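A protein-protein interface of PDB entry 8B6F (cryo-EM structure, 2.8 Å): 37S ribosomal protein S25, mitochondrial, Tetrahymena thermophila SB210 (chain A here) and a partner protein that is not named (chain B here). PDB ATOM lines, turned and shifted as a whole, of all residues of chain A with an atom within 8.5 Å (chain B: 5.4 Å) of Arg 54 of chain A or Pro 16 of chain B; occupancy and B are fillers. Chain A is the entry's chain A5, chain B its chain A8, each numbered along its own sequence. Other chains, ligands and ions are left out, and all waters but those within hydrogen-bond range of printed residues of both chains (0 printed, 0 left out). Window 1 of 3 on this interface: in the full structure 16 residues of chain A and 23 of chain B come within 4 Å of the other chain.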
ATOM      1  N   THR A  51      22.244  15.209 -16.067  1.00  0.00           N
ATOM      2  CA  THR A  51      22.533  14.840 -14.689  1.00  0.00           C
ATOM      3  C   THR A  51      23.860  14.097 -14.612  1.00  0.00           C
ATOM      4  O   THR A  51      24.157  13.230 -15.439  1.00  0.00           O
ATOM      5  CB  THR A  51      21.410  13.968 -14.127  1.00  0.00           C
ATOM      6  OG1 THR A  51      20.152  14.635 -14.291  1.00  0.00           O
ATOM      7  CG2 THR A  51      21.635  13.689 -12.647  1.00  0.00           C
ATOM      8  N   ALA A  52      24.659  14.441 -13.606  1.00  0.00           N
ATOM      9  CA  ALA A  52      25.974  13.837 -13.455  1.00  0.00           C
ATOM     10  C   ALA A  52      25.844  12.347 -13.166  1.00  0.00           C
ATOM     11  O   ALA A  52      24.858  11.886 -12.588  1.00  0.00           O
ATOM     12  CB  ALA A  52      26.747  14.525 -12.331  1.00  0.00           C
ATOM     13  N   PHE A  53      26.860  11.588 -13.578  1.00  0.00           N
ATOM     14  CA  PHE A  53      26.829  10.145 -13.373  1.00  0.00           C
ATOM     15  C   PHE A  53      26.742   9.806 -11.892  1.00  0.00           C
ATOM     16  O   PHE A  53      25.984   8.913 -11.496  1.00  0.00           O
ATOM     17  CB  PHE A  53      28.067   9.504 -14.000  1.00  0.00           C
ATOM     18  CG  PHE A  53      28.213   8.042 -13.693  1.00  0.00           C
ATOM     19  CD1 PHE A  53      27.473   7.098 -14.383  1.00  0.00           C
ATOM     20  CD2 PHE A  53      29.102   7.611 -12.724  1.00  0.00           C
ATOM     21  CE1 PHE A  53      27.610   5.753 -14.105  1.00  0.00           C
ATOM     22  CE2 PHE A  53      29.244   6.268 -12.442  1.00  0.00           C
ATOM     23  CZ  PHE A  53      28.497   5.337 -13.133  1.00  0.00           C
ATOM     24  N   ARG A  54      27.502  10.514 -11.057  1.00  0.00           N
ATOM     25  CA  ARG A  54      27.463  10.266  -9.620  1.00  0.00           C
ATOM     26  C   ARG A  54      26.077  10.494  -9.031  1.00  0.00           C
ATOM     27  O   ARG A  54      25.782   9.966  -7.954  1.00  0.00           O
ATOM     28  CB  ARG A  54      28.484  11.157  -8.909  1.00  0.00           C
ATOM     29  CG  ARG A  54      28.273  12.641  -9.154  1.00  0.00           C
ATOM     30  CD  ARG A  54      29.358  13.483  -8.511  1.00  0.00           C
ATOM     31  NE  ARG A  54      29.376  13.353  -7.060  1.00  0.00           N
ATOM     32  CZ  ARG A  54      30.019  14.177  -6.245  1.00  0.00           C
ATOM     33  NH1 ARG A  54      30.690  15.220  -6.703  1.00  0.00           N
ATOM     34  NH2 ARG A  54      29.986  13.950  -4.935  1.00  0.00           N
ATOM     35  N   ASP A  55      25.224  11.267  -9.706  1.00  0.00           N
ATOM     36  CA  ASP A  55      23.868  11.530  -9.245  1.00  0.00           C
ATOM     37  C   ASP A  55      22.796  10.862 -10.092  1.00  0.00           C
ATOM     38  O   ASP A  55      21.621  10.906  -9.717  1.00  0.00           O
ATOM     39  CB  ASP A  55      23.604  13.042  -9.219  1.00  0.00           C
ATOM     40  CG  ASP A  55      24.545  13.783  -8.296  1.00  0.00           C
ATOM     41  OD1 ASP A  55      25.302  13.118  -7.561  1.00  0.00           O
ATOM     42  OD2 ASP A  55      24.530  15.031  -8.308  1.00  0.00           O
ATOM     43  N   SER A  56      23.161  10.254 -11.213  1.00  0.00           N
ATOM     44  CA  SER A  56      22.197   9.688 -12.142  1.00  0.00           C
ATOM     45  C   SER A  56      21.690   8.343 -11.648  1.00  0.00           C
ATOM     46  O   SER A  56      22.268   7.733 -10.748  1.00  0.00           O
ATOM     47  CB  SER A  56      22.848   9.496 -13.504  1.00  0.00           C
ATOM     48  OG  SER A  56      23.839   8.491 -13.390  1.00  0.00           O
ATOM     49  N   PRO A  57      20.591   7.845 -12.224  1.00  0.00           N
ATOM     50  CA  PRO A  57      20.121   6.496 -11.875  1.00  0.00           C
ATOM     51  C   PRO A  57      21.038   5.382 -12.354  1.00  0.00           C
ATOM     52  O   PRO A  57      20.744   4.210 -12.094  1.00  0.00           O
ATOM     53  CB  PRO A  57      18.753   6.406 -12.574  1.00  0.00           C
ATOM     54  CG  PRO A  57      18.405   7.795 -12.982  1.00  0.00           C
ATOM     55  CD  PRO A  57      19.693   8.507 -13.185  1.00  0.00           C
ATOM     56  N   HIS A  58      22.130   5.701 -13.050  1.00  0.00           N
ATOM     57  CA  HIS A  58      23.043   4.704 -13.595  1.00  0.00           C
ATOM     58  C   HIS A  58      24.242   4.450 -12.694  1.00  0.00           C
ATOM     59  O   HIS A  58      25.202   3.807 -13.128  1.00  0.00           O
ATOM     60  CB  HIS A  58      23.528   5.137 -14.980  1.00  0.00           C
ATOM     61  CG  HIS A  58      22.423   5.460 -15.933  1.00  0.00           C
ATOM     62  ND1 HIS A  58      21.744   4.493 -16.644  1.00  0.00           N
ATOM     63  CD2 HIS A  58      21.879   6.645 -16.299  1.00  0.00           C
ATOM     64  CE1 HIS A  58      20.829   5.068 -17.403  1.00  0.00           C
ATOM     65  NE2 HIS A  58      20.890   6.374 -17.212  1.00  0.00           N
ATOM     66  N   ASN A  59      24.220   4.945 -11.463  1.00  0.00           N
ATOM     67  CA  ASN A  59      25.308   4.758 -10.507  1.00  0.00           C
ATOM     68  C   ASN A  59      24.795   3.855  -9.388  1.00  0.00           C
ATOM     69  O   ASN A  59      24.271   4.328  -8.379  1.00  0.00           O
ATOM     70  CB  ASN A  59      25.794   6.098  -9.971  1.00  0.00           C
ATOM     71  CG  ASN A  59      26.950   5.953  -9.008  1.00  0.00           C
ATOM     72  OD1 ASN A  59      27.723   5.000  -9.089  1.00  0.00           O
ATOM     73  ND2 ASN A  59      27.072   6.898  -8.085  1.00  0.00           N
ATOM     74  N   ILE A  60      24.952   2.543  -9.575  1.00  0.00           N
ATOM     75  CA  ILE A  60      24.503   1.587  -8.568  1.00  0.00           C
ATOM     76  C   ILE A  60      25.614   1.187  -7.605  1.00  0.00           C
ATOM     77  O   ILE A  60      25.318   0.736  -6.489  1.00  0.00           O
ATOM     78  CB  ILE A  60      23.885   0.335  -9.226  1.00  0.00           C
ATOM     79  CG1 ILE A  60      24.838  -0.370 -10.205  1.00  0.00           C
ATOM     80  CG2 ILE A  60      22.600   0.703  -9.944  1.00  0.00           C
ATOM     81  CD1 ILE A  60      25.909  -1.231  -9.576  1.00  0.00           C
ATOM     82  N   ARG A  61      26.875   1.334  -7.997  1.00  0.00           N
ATOM     83  CA  ARG A  61      27.966   1.097  -7.065  1.00  0.00           C
ATOM     84  C   ARG A  61      27.889   2.098  -5.923  1.00  0.00           C
ATOM     85  O   ARG A  61      27.499   3.254  -6.114  1.00  0.00           O
ATOM     86  CB  ARG A  61      29.311   1.203  -7.781  1.00  0.00           C
ATOM     87  CG  ARG A  61      30.501   0.833  -6.912  1.00  0.00           C
ATOM     88  CD  ARG A  61      31.815   1.020  -7.650  1.00  0.00           C
ATOM     89  NE  ARG A  61      31.926   0.144  -8.810  1.00  0.00           N
ATOM     90  CZ  ARG A  61      32.983   0.088  -9.609  1.00  0.00           C
ATOM     91  NH1 ARG A  61      34.049   0.844  -9.401  1.00  0.00           N
ATOM     92  NH2 ARG A  61      32.972  -0.748 -10.643  1.00  0.00           N
ATOM     93  N   TYR A  62      28.255   1.648  -4.728  1.00  0.00           N
ATOM     94  CA  TYR A  62      28.158   2.417  -3.492  1.00  0.00           C
ATOM     95  C   TYR A  62      26.717   2.616  -3.046  1.00  0.00           C
ATOM     96  O   TYR A  62      26.462   3.421  -2.143  1.00  0.00           O
ATOM     97  CB  TYR A  62      28.842   3.784  -3.615  1.00  0.00           C
ATOM     98  CG  TYR A  62      30.278   3.697  -4.072  1.00  0.00           C
ATOM     99  CD1 TYR A  62      31.265   3.199  -3.232  1.00  0.00           C
ATOM    100  CD2 TYR A  62      30.649   4.121  -5.341  1.00  0.00           C
ATOM    101  CE1 TYR A  62      32.580   3.118  -3.646  1.00  0.00           C
ATOM    102  CE2 TYR A  62      31.961   4.045  -5.763  1.00  0.00           C
ATOM    103  CZ  TYR A  62      32.921   3.542  -4.912  1.00  0.00           C
ATOM    104  OH  TYR A  62      34.229   3.465  -5.327  1.00  0.00           O
ATOM    105  N   GLU A  65      25.934   0.840   1.941  1.00  0.00           N
ATOM    106  CA  GLU A  65      26.772   1.693   2.774  1.00  0.00           C
ATOM    107  C   GLU A  65      28.029   0.927   3.166  1.00  0.00           C
ATOM    108  O   GLU A  65      27.972   0.002   3.982  1.00  0.00           O
ATOM    109  CB  GLU A  65      25.999   2.156   4.004  1.00  0.00           C
ATOM    110  CG  GLU A  65      24.661   2.795   3.673  1.00  0.00           C
ATOM    111  CD  GLU A  65      23.916   3.262   4.905  1.00  0.00           C
ATOM    112  OE1 GLU A  65      24.550   3.370   5.974  1.00  0.00           O
ATOM    113  OE2 GLU A  65      22.697   3.514   4.805  1.00  0.00           O
ATOM    114  N   ILE A  66      29.168   1.310   2.586  1.00  0.00           N
ATOM    115  CA  ILE A  66      30.423   0.640   2.912  1.00  0.00           C
ATOM    116  C   ILE A  66      30.841   0.959   4.344  1.00  0.00           C
ATOM    117  O   ILE A  66      31.375   0.098   5.053  1.00  0.00           O
ATOM    118  CB  ILE A  66      31.520   1.023   1.902  1.00  0.00           C
ATOM    119  CG1 ILE A  66      31.828   2.522   1.983  1.00  0.00           C
ATOM    120  CG2 ILE A  66      31.088   0.624   0.495  1.00  0.00           C
ATOM    121  CD1 ILE A  66      32.875   3.001   0.998  1.00  0.00           C
ATOM    122  N   HIS A  67      30.611   2.191   4.789  1.00  0.00           N
ATOM    123  CA  HIS A  67      30.926   2.608   6.150  1.00  0.00           C
ATOM    124  C   HIS A  67      29.663   2.515   6.996  1.00  0.00           C
ATOM    125  O   HIS A  67      28.648   3.141   6.673  1.00  0.00           O
ATOM    126  CB  HIS A  67      31.484   4.030   6.176  1.00  0.00           C
ATOM    127  CG  HIS A  67      32.842   4.156   5.558  1.00  0.00           C
ATOM    128  ND1 HIS A  67      33.046   4.711   4.313  1.00  0.00           N
ATOM    129  CD2 HIS A  67      34.064   3.791   6.012  1.00  0.00           C
ATOM    130  CE1 HIS A  67      34.335   4.684   4.028  1.00  0.00           C
ATOM    131  NE2 HIS A  67      34.976   4.131   5.042  1.00  0.00           N
ATOM    132  N   TYR B  13      37.893  15.661  -4.238  1.00  0.00           N
ATOM    133  CA  TYR B  13      36.874  16.149  -3.323  1.00  0.00           C
ATOM    134  C   TYR B  13      36.217  14.967  -2.628  1.00  0.00           C
ATOM    135  O   TYR B  13      36.111  13.876  -3.194  1.00  0.00           O
ATOM    136  CB  TYR B  13      35.823  16.985  -4.058  1.00  0.00           C
ATOM    137  CG  TYR B  13      35.291  16.320  -5.302  1.00  0.00           C
ATOM    138  CD1 TYR B  13      34.198  15.467  -5.245  1.00  0.00           C
ATOM    139  CD2 TYR B  13      35.889  16.541  -6.535  1.00  0.00           C
ATOM    140  CE1 TYR B  13      33.712  14.856  -6.384  1.00  0.00           C
ATOM    141  CE2 TYR B  13      35.411  15.934  -7.679  1.00  0.00           C
ATOM    142  CZ  TYR B  13      34.322  15.093  -7.596  1.00  0.00           C
ATOM    143  OH  TYR B  13      33.843  14.488  -8.734  1.00  0.00           O
ATOM    144  N   LEU B  14      35.778  15.196  -1.395  1.00  0.00           N
ATOM    145  CA  LEU B  14      35.107  14.158  -0.628  1.00  0.00           C
ATOM    146  C   LEU B  14      33.722  13.885  -1.203  1.00  0.00           C
ATOM    147  O   LEU B  14      33.097  14.751  -1.821  1.00  0.00           O
ATOM    148  CB  LEU B  14      34.998  14.576   0.838  1.00  0.00           C
ATOM    149  CG  LEU B  14      34.386  13.568   1.810  1.00  0.00           C
ATOM    150  CD1 LEU B  14      35.214  12.295   1.857  1.00  0.00           C
ATOM    151  CD2 LEU B  14      34.263  14.177   3.192  1.00  0.00           C
ATOM    152  N   GLN B  15      33.238  12.664  -0.988  1.00  0.00           N
ATOM    153  CA  GLN B  15      31.946  12.237  -1.495  1.00  0.00           C
ATOM    154  C   GLN B  15      31.076  11.719  -0.361  1.00  0.00           C
ATOM    155  O   GLN B  15      31.588  11.208   0.639  1.00  0.00           O
ATOM    156  CB  GLN B  15      32.108  11.142  -2.560  1.00  0.00           C
ATOM    157  CG  GLN B  15      32.670  11.656  -3.874  1.00  0.00           C
ATOM    158  CD  GLN B  15      32.938  10.546  -4.865  1.00  0.00           C
ATOM    159  OE1 GLN B  15      33.243   9.418  -4.483  1.00  0.00           O
ATOM    160  NE2 GLN B  15      32.819  10.860  -6.148  1.00  0.00           N
ATOM    161  N   PRO B  16      29.752  11.839  -0.491  1.00  0.00           N
ATOM    162  CA  PRO B  16      28.878  11.461   0.632  1.00  0.00           C
ATOM    163  C   PRO B  16      29.001  10.005   1.044  1.00  0.00           C
ATOM    164  O   PRO B  16      28.897   9.698   2.238  1.00  0.00           O
ATOM    165  CB  PRO B  16      27.474  11.790   0.102  1.00  0.00           C
ATOM    166  CG  PRO B  16      27.606  11.763  -1.376  1.00  0.00           C
ATOM    167  CD  PRO B  16      28.981  12.266  -1.670  1.00  0.00           C
ATOM    168  N   TRP B  17      29.220   9.094   0.095  1.00  0.00           N
ATOM    169  CA  TRP B  17      29.268   7.679   0.441  1.00  0.00           C
ATOM    170  C   TRP B  17      30.521   7.315   1.224  1.00  0.00           C
ATOM    171  O   TRP B  17      30.536   6.276   1.889  1.00  0.00           O
ATOM    172  CB  TRP B  17      29.171   6.817  -0.821  1.00  0.00           C
ATOM    173  CG  TRP B  17      30.255   7.058  -1.823  1.00  0.00           C
ATOM    174  CD1 TRP B  17      30.185   7.858  -2.924  1.00  0.00           C
ATOM    175  CD2 TRP B  17      31.568   6.484  -1.827  1.00  0.00           C
ATOM    176  NE1 TRP B  17      31.374   7.823  -3.611  1.00  0.00           N
ATOM    177  CE2 TRP B  17      32.239   6.987  -2.958  1.00  0.00           C
ATOM    178  CE3 TRP B  17      32.241   5.597  -0.981  1.00  0.00           C
ATOM    179  CZ2 TRP B  17      33.551   6.634  -3.265  1.00  0.00           C
ATOM    180  CZ3 TRP B  17      33.546   5.247  -1.289  1.00  0.00           C
ATOM    181  CH2 TRP B  17      34.186   5.765  -2.422  1.00  0.00           C
ATOM    182  N   GLU B  18      31.568   8.139   1.160  1.00  0.00           N
ATOM    183  CA  GLU B  18      32.759   7.870   1.959  1.00  0.00           C
ATOM    184  C   GLU B  18      32.478   8.053   3.443  1.00  0.00           C
ATOM    185  O   GLU B  18      32.964   7.277   4.274  1.00  0.00           O
ATOM    186  CB  GLU B  18      33.904   8.779   1.517  1.00  0.00           C
ATOM    187  CG  GLU B  18      34.247   8.655   0.043  1.00  0.00           C
ATOM    188  CD  GLU B  18      35.508   9.409  -0.323  1.00  0.00           C
ATOM    189  OE1 GLU B  18      36.287   9.739   0.592  1.00  0.00           O
ATOM    190  OE2 GLU B  18      35.719   9.669  -1.525  1.00  0.00           O
ATOM    191  N   LEU B  19      31.704   9.073   3.797  1.00  0.00           N
ATOM    192  CA  LEU B  19      31.352   9.316   5.184  1.00  0.00           C
ATOM    193  C   LEU B  19      30.257   8.358   5.637  1.00  0.00           C
ATOM    194  O   LEU B  19      29.497   7.814   4.832  1.00  0.00           O
ATOM    195  CB  LEU B  19      30.880  10.758   5.373  1.00  0.00           C
ATOM    196  CG  LEU B  19      31.890  11.852   5.036  1.00  0.00           C
ATOM    197  CD1 LEU B  19      31.217  13.209   5.079  1.00  0.00           C
ATOM    198  CD2 LEU B  19      33.071  11.807   5.994  1.00  0.00           C
ATOM    199  N   GLU B  20      30.182   8.158   6.948  1.00  0.00           N
ATOM    200  CA  GLU B  20      29.074   7.412   7.520  1.00  0.00           C
ATOM    201  C   GLU B  20      27.776   8.186   7.339  1.00  0.00           C
ATOM    202  O   GLU B  20      27.755   9.419   7.339  1.00  0.00           O
ATOM    203  CB  GLU B  20      29.317   7.139   9.004  1.00  0.00           C
ATOM    204  CG  GLU B  20      30.494   6.219   9.269  1.00  0.00           C
ATOM    205  CD  GLU B  20      30.675   5.918  10.742  1.00  0.00           C
ATOM    206  OE1 GLU B  20      29.895   6.454  11.557  1.00  0.00           O
ATOM    207  OE2 GLU B  20      31.596   5.148  11.086  1.00  0.00           O
ATOM    208  N   TYR B  24      26.849  12.346   7.846  1.00  0.00           N
ATOM    209  CA  TYR B  24      26.301  13.159   6.767  1.00  0.00           C
ATOM    210  C   TYR B  24      24.965  13.769   7.169  1.00  0.00           C
ATOM    211  O   TYR B  24      24.729  14.966   6.977  1.00  0.00           O
ATOM    212  CB  TYR B  24      26.153  12.304   5.509  1.00  0.00           C
ATOM    213  CG  TYR B  24      25.766  13.072   4.268  1.00  0.00           C
ATOM    214  CD1 TYR B  24      26.724  13.731   3.510  1.00  0.00           C
ATOM    215  CD2 TYR B  24      24.448  13.113   3.837  1.00  0.00           C
ATOM    216  CE1 TYR B  24      26.379  14.425   2.371  1.00  0.00           C
ATOM    217  CE2 TYR B  24      24.092  13.805   2.699  1.00  0.00           C
ATOM    218  CZ  TYR B  24      25.064  14.457   1.970  1.00  0.00           C
ATOM    219  OH  TYR B  24      24.715  15.146   0.834  1.00  0.00           O
ATOM    220  N   THR B  52      30.961  18.434   2.411  1.00  0.00           N
ATOM    221  CA  THR B  52      30.819  17.955   1.046  1.00  0.00           C
ATOM    222  C   THR B  52      30.240  19.071   0.186  1.00  0.00           C
ATOM    223  O   THR B  52      29.594  19.995   0.684  1.00  0.00           O
ATOM    224  CB  THR B  52      29.915  16.710   0.989  1.00  0.00           C
ATOM    225  OG1 THR B  52      30.410  15.713   1.890  1.00  0.00           O
ATOM    226  CG2 THR B  52      29.859  16.126  -0.410  1.00  0.00           C
ATOM    227  N   ASP B  53      30.479  18.973  -1.123  1.00  0.00           N
ATOM    228  CA  ASP B  53      29.981  19.994  -2.037  1.00  0.00           C
ATOM    229  C   ASP B  53      28.459  20.069  -2.002  1.00  0.00           C
ATOM    230  O   ASP B  53      27.886  21.162  -2.062  1.00  0.00           O
ATOM    231  CB  ASP B  53      30.481  19.727  -3.458  1.00  0.00           C
ATOM    232  CG  ASP B  53      30.193  18.315  -3.928  1.00  0.00           C
ATOM    233  OD1 ASP B  53      30.308  17.378  -3.114  1.00  0.00           O
ATOM    234  OD2 ASP B  53      29.852  18.142  -5.117  1.00  0.00           O
ATOM    235  N   TYR B  54      27.787  18.921  -1.906  1.00  0.00           N
ATOM    236  CA  TYR B  54      26.333  18.930  -1.783  1.00  0.00           C
ATOM    237  C   TYR B  54      25.895  19.745  -0.575  1.00  0.00           C
ATOM    238  O   TYR B  54      24.983  20.575  -0.665  1.00  0.00           O
ATOM    239  CB  TYR B  54      25.804  17.501  -1.664  1.00  0.00           C
ATOM    240  CG  TYR B  54      26.037  16.640  -2.879  1.00  0.00           C
ATOM    241  CD1 TYR B  54      25.336  16.862  -4.054  1.00  0.00           C
ATOM    242  CD2 TYR B  54      26.938  15.588  -2.843  1.00  0.00           C
ATOM    243  CE1 TYR B  54      25.536  16.072  -5.165  1.00  0.00           C
ATOM    244  CE2 TYR B  54      27.148  14.791  -3.947  1.00  0.00           C
ATOM    245  CZ  TYR B  54      26.444  15.037  -5.106  1.00  0.00           C
ATOM    246  OH  TYR B  54      26.649  14.247  -6.210  1.00  0.00           O
ATOM    247  N   GLU B  92      31.746  16.384 -12.873  1.00  0.00           N
ATOM    248  CA  GLU B  92      30.708  15.727 -12.089  1.00  0.00           C
ATOM    249  C   GLU B  92      30.130  16.622 -11.002  1.00  0.00           C
ATOM    250  O   GLU B  92      29.105  16.263 -10.414  1.00  0.00           O
ATOM    251  CB  GLU B  92      31.255  14.444 -11.465  1.00  0.00           C
ATOM    252  CG  GLU B  92      31.621  13.378 -12.485  1.00  0.00           C
ATOM    253  CD  GLU B  92      32.023  12.064 -11.839  1.00  0.00           C
ATOM    254  OE1 GLU B  92      32.243  12.045 -10.611  1.00  0.00           O
ATOM    255  OE2 GLU B  92      32.114  11.047 -12.561  1.00  0.00           O
ATOM    256  N   CYS B  93      30.754  17.767 -10.721  1.00  0.00           N
ATOM    257  CA  CYS B  93      30.232  18.724  -9.752  1.00  0.00           C
ATOM    258  C   CYS B  93      29.384  19.807 -10.406  1.00  0.00           C
ATOM    259  O   CYS B  93      29.292  20.922  -9.879  1.00  0.00           O
ATOM    260  CB  CYS B  93      31.384  19.353  -8.969  1.00  0.00           C
ATOM    261  SG  CYS B  93      32.313  18.187  -7.948  1.00  0.00           S
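NH1 of Arg 54 of chain A lies within salt-bridge range of OD2 of Asp 53 of chain B (3.4 Å). The side-chain hydroxyl of Tyr 54 of chain B sits at hydrogen-bond distance from the guanidinium group of Arg 54 of chain A. NH1 of Arg 54 of chain A is in hydrogen-bond range of SG of Cys 93 of chain B. The side-chain hydroxyl (OH) of Tyr 54 of chain B lies close to the side-chain carboxylate (OD2) of Asp 55 of chain A, 3.1 Å away. A ring nitrogen (ND1) of His 67 of chain A is in hydrogen-bond range of the backbone carbonyl oxygen (O) of Glu 18 of chain B, 2.6 Å away.
Printed residues of chain A that touch a printed residue of chain B: Ala 52, Arg 54, Asp 55, Tyr 62, Ile 66 and His 67. Of the 14 printed residues of chain B, 10 touch a printed residue of chain A. Hydrophobic or aromatic side chains of chain B that line the printed part of chain A: Tyr 13, Pro 16, Trp 17 and Tyr 54. Among the printed residues, 14 pairs touch across the chains. Among the printed residues, Asp or Glu carboxylates within 4 Å of a Lys or Arg side-chain nitrogen of the other chain: Arg 54 of chain A with Asp 53 of chain B.
Printed residues of chain B within 4 Å of Arg 54 of chain A: Tyr 13, Gln 15, Pro 16, Asp 53, Tyr 54, Glu 92 and Cys 93. Of the printed residues of chain B, Asp 55 of chain A touches Tyr 54. Of the printed residues of chain A, Gln 15 of chain B touches Arg 54 (3.7 Å). Pro 16 of chain B touches just one residue of chain A: Arg 54. The nearest residue of chain B that does not touch Arg 54 of chain A is Leu 14 of chain B (4.5 Å). The nearest residue of chain A that does not touch Pro 16 of chain B is Asp 55 of chain A (6.7 Å).
Among the printed residues, merely in contact across the chains: Ala 52 of chain A with Glu 92 of chain B (3.5 Å), Arg 54 of chain A with Tyr 13 of chain B (3.1 Å), Arg 54 of chain A with Gln 15 of chain B (3.7 Å), Arg 54 of chain A with Pro 16 of chain B (3.8 Å), Arg 54 of chain A with Glu 92 of chain B (3.4 Å), Tyr 62 of chain A with Trp 17 of chain B (3.3 Å), Ile 66 of chain A with Trp 17 of chain B (3.3 Å), His 67 of chain A with Trp 17 of chain B (3.8 Å) and His 67 of chain A with Glu 20 of chain B (3.9 Å).
ND2 of Asn 59 of chain A lies within hydrogen-bond range of O of Arg 54 of chain A, 3.3 Å away. OH of Tyr 13 of chain B sits at hydrogen-bond distance from OE1 of Glu 92 of chain B, 3.5 Å away. The side-chain amide oxygen of Gln 15 of chain B is in hydrogen-bond range of the indole nitrogen of Trp 17 of chain B. SG of Cys 93 of chain B sits at hydrogen-bond distance from OD2 of Asp 53 of chain B.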
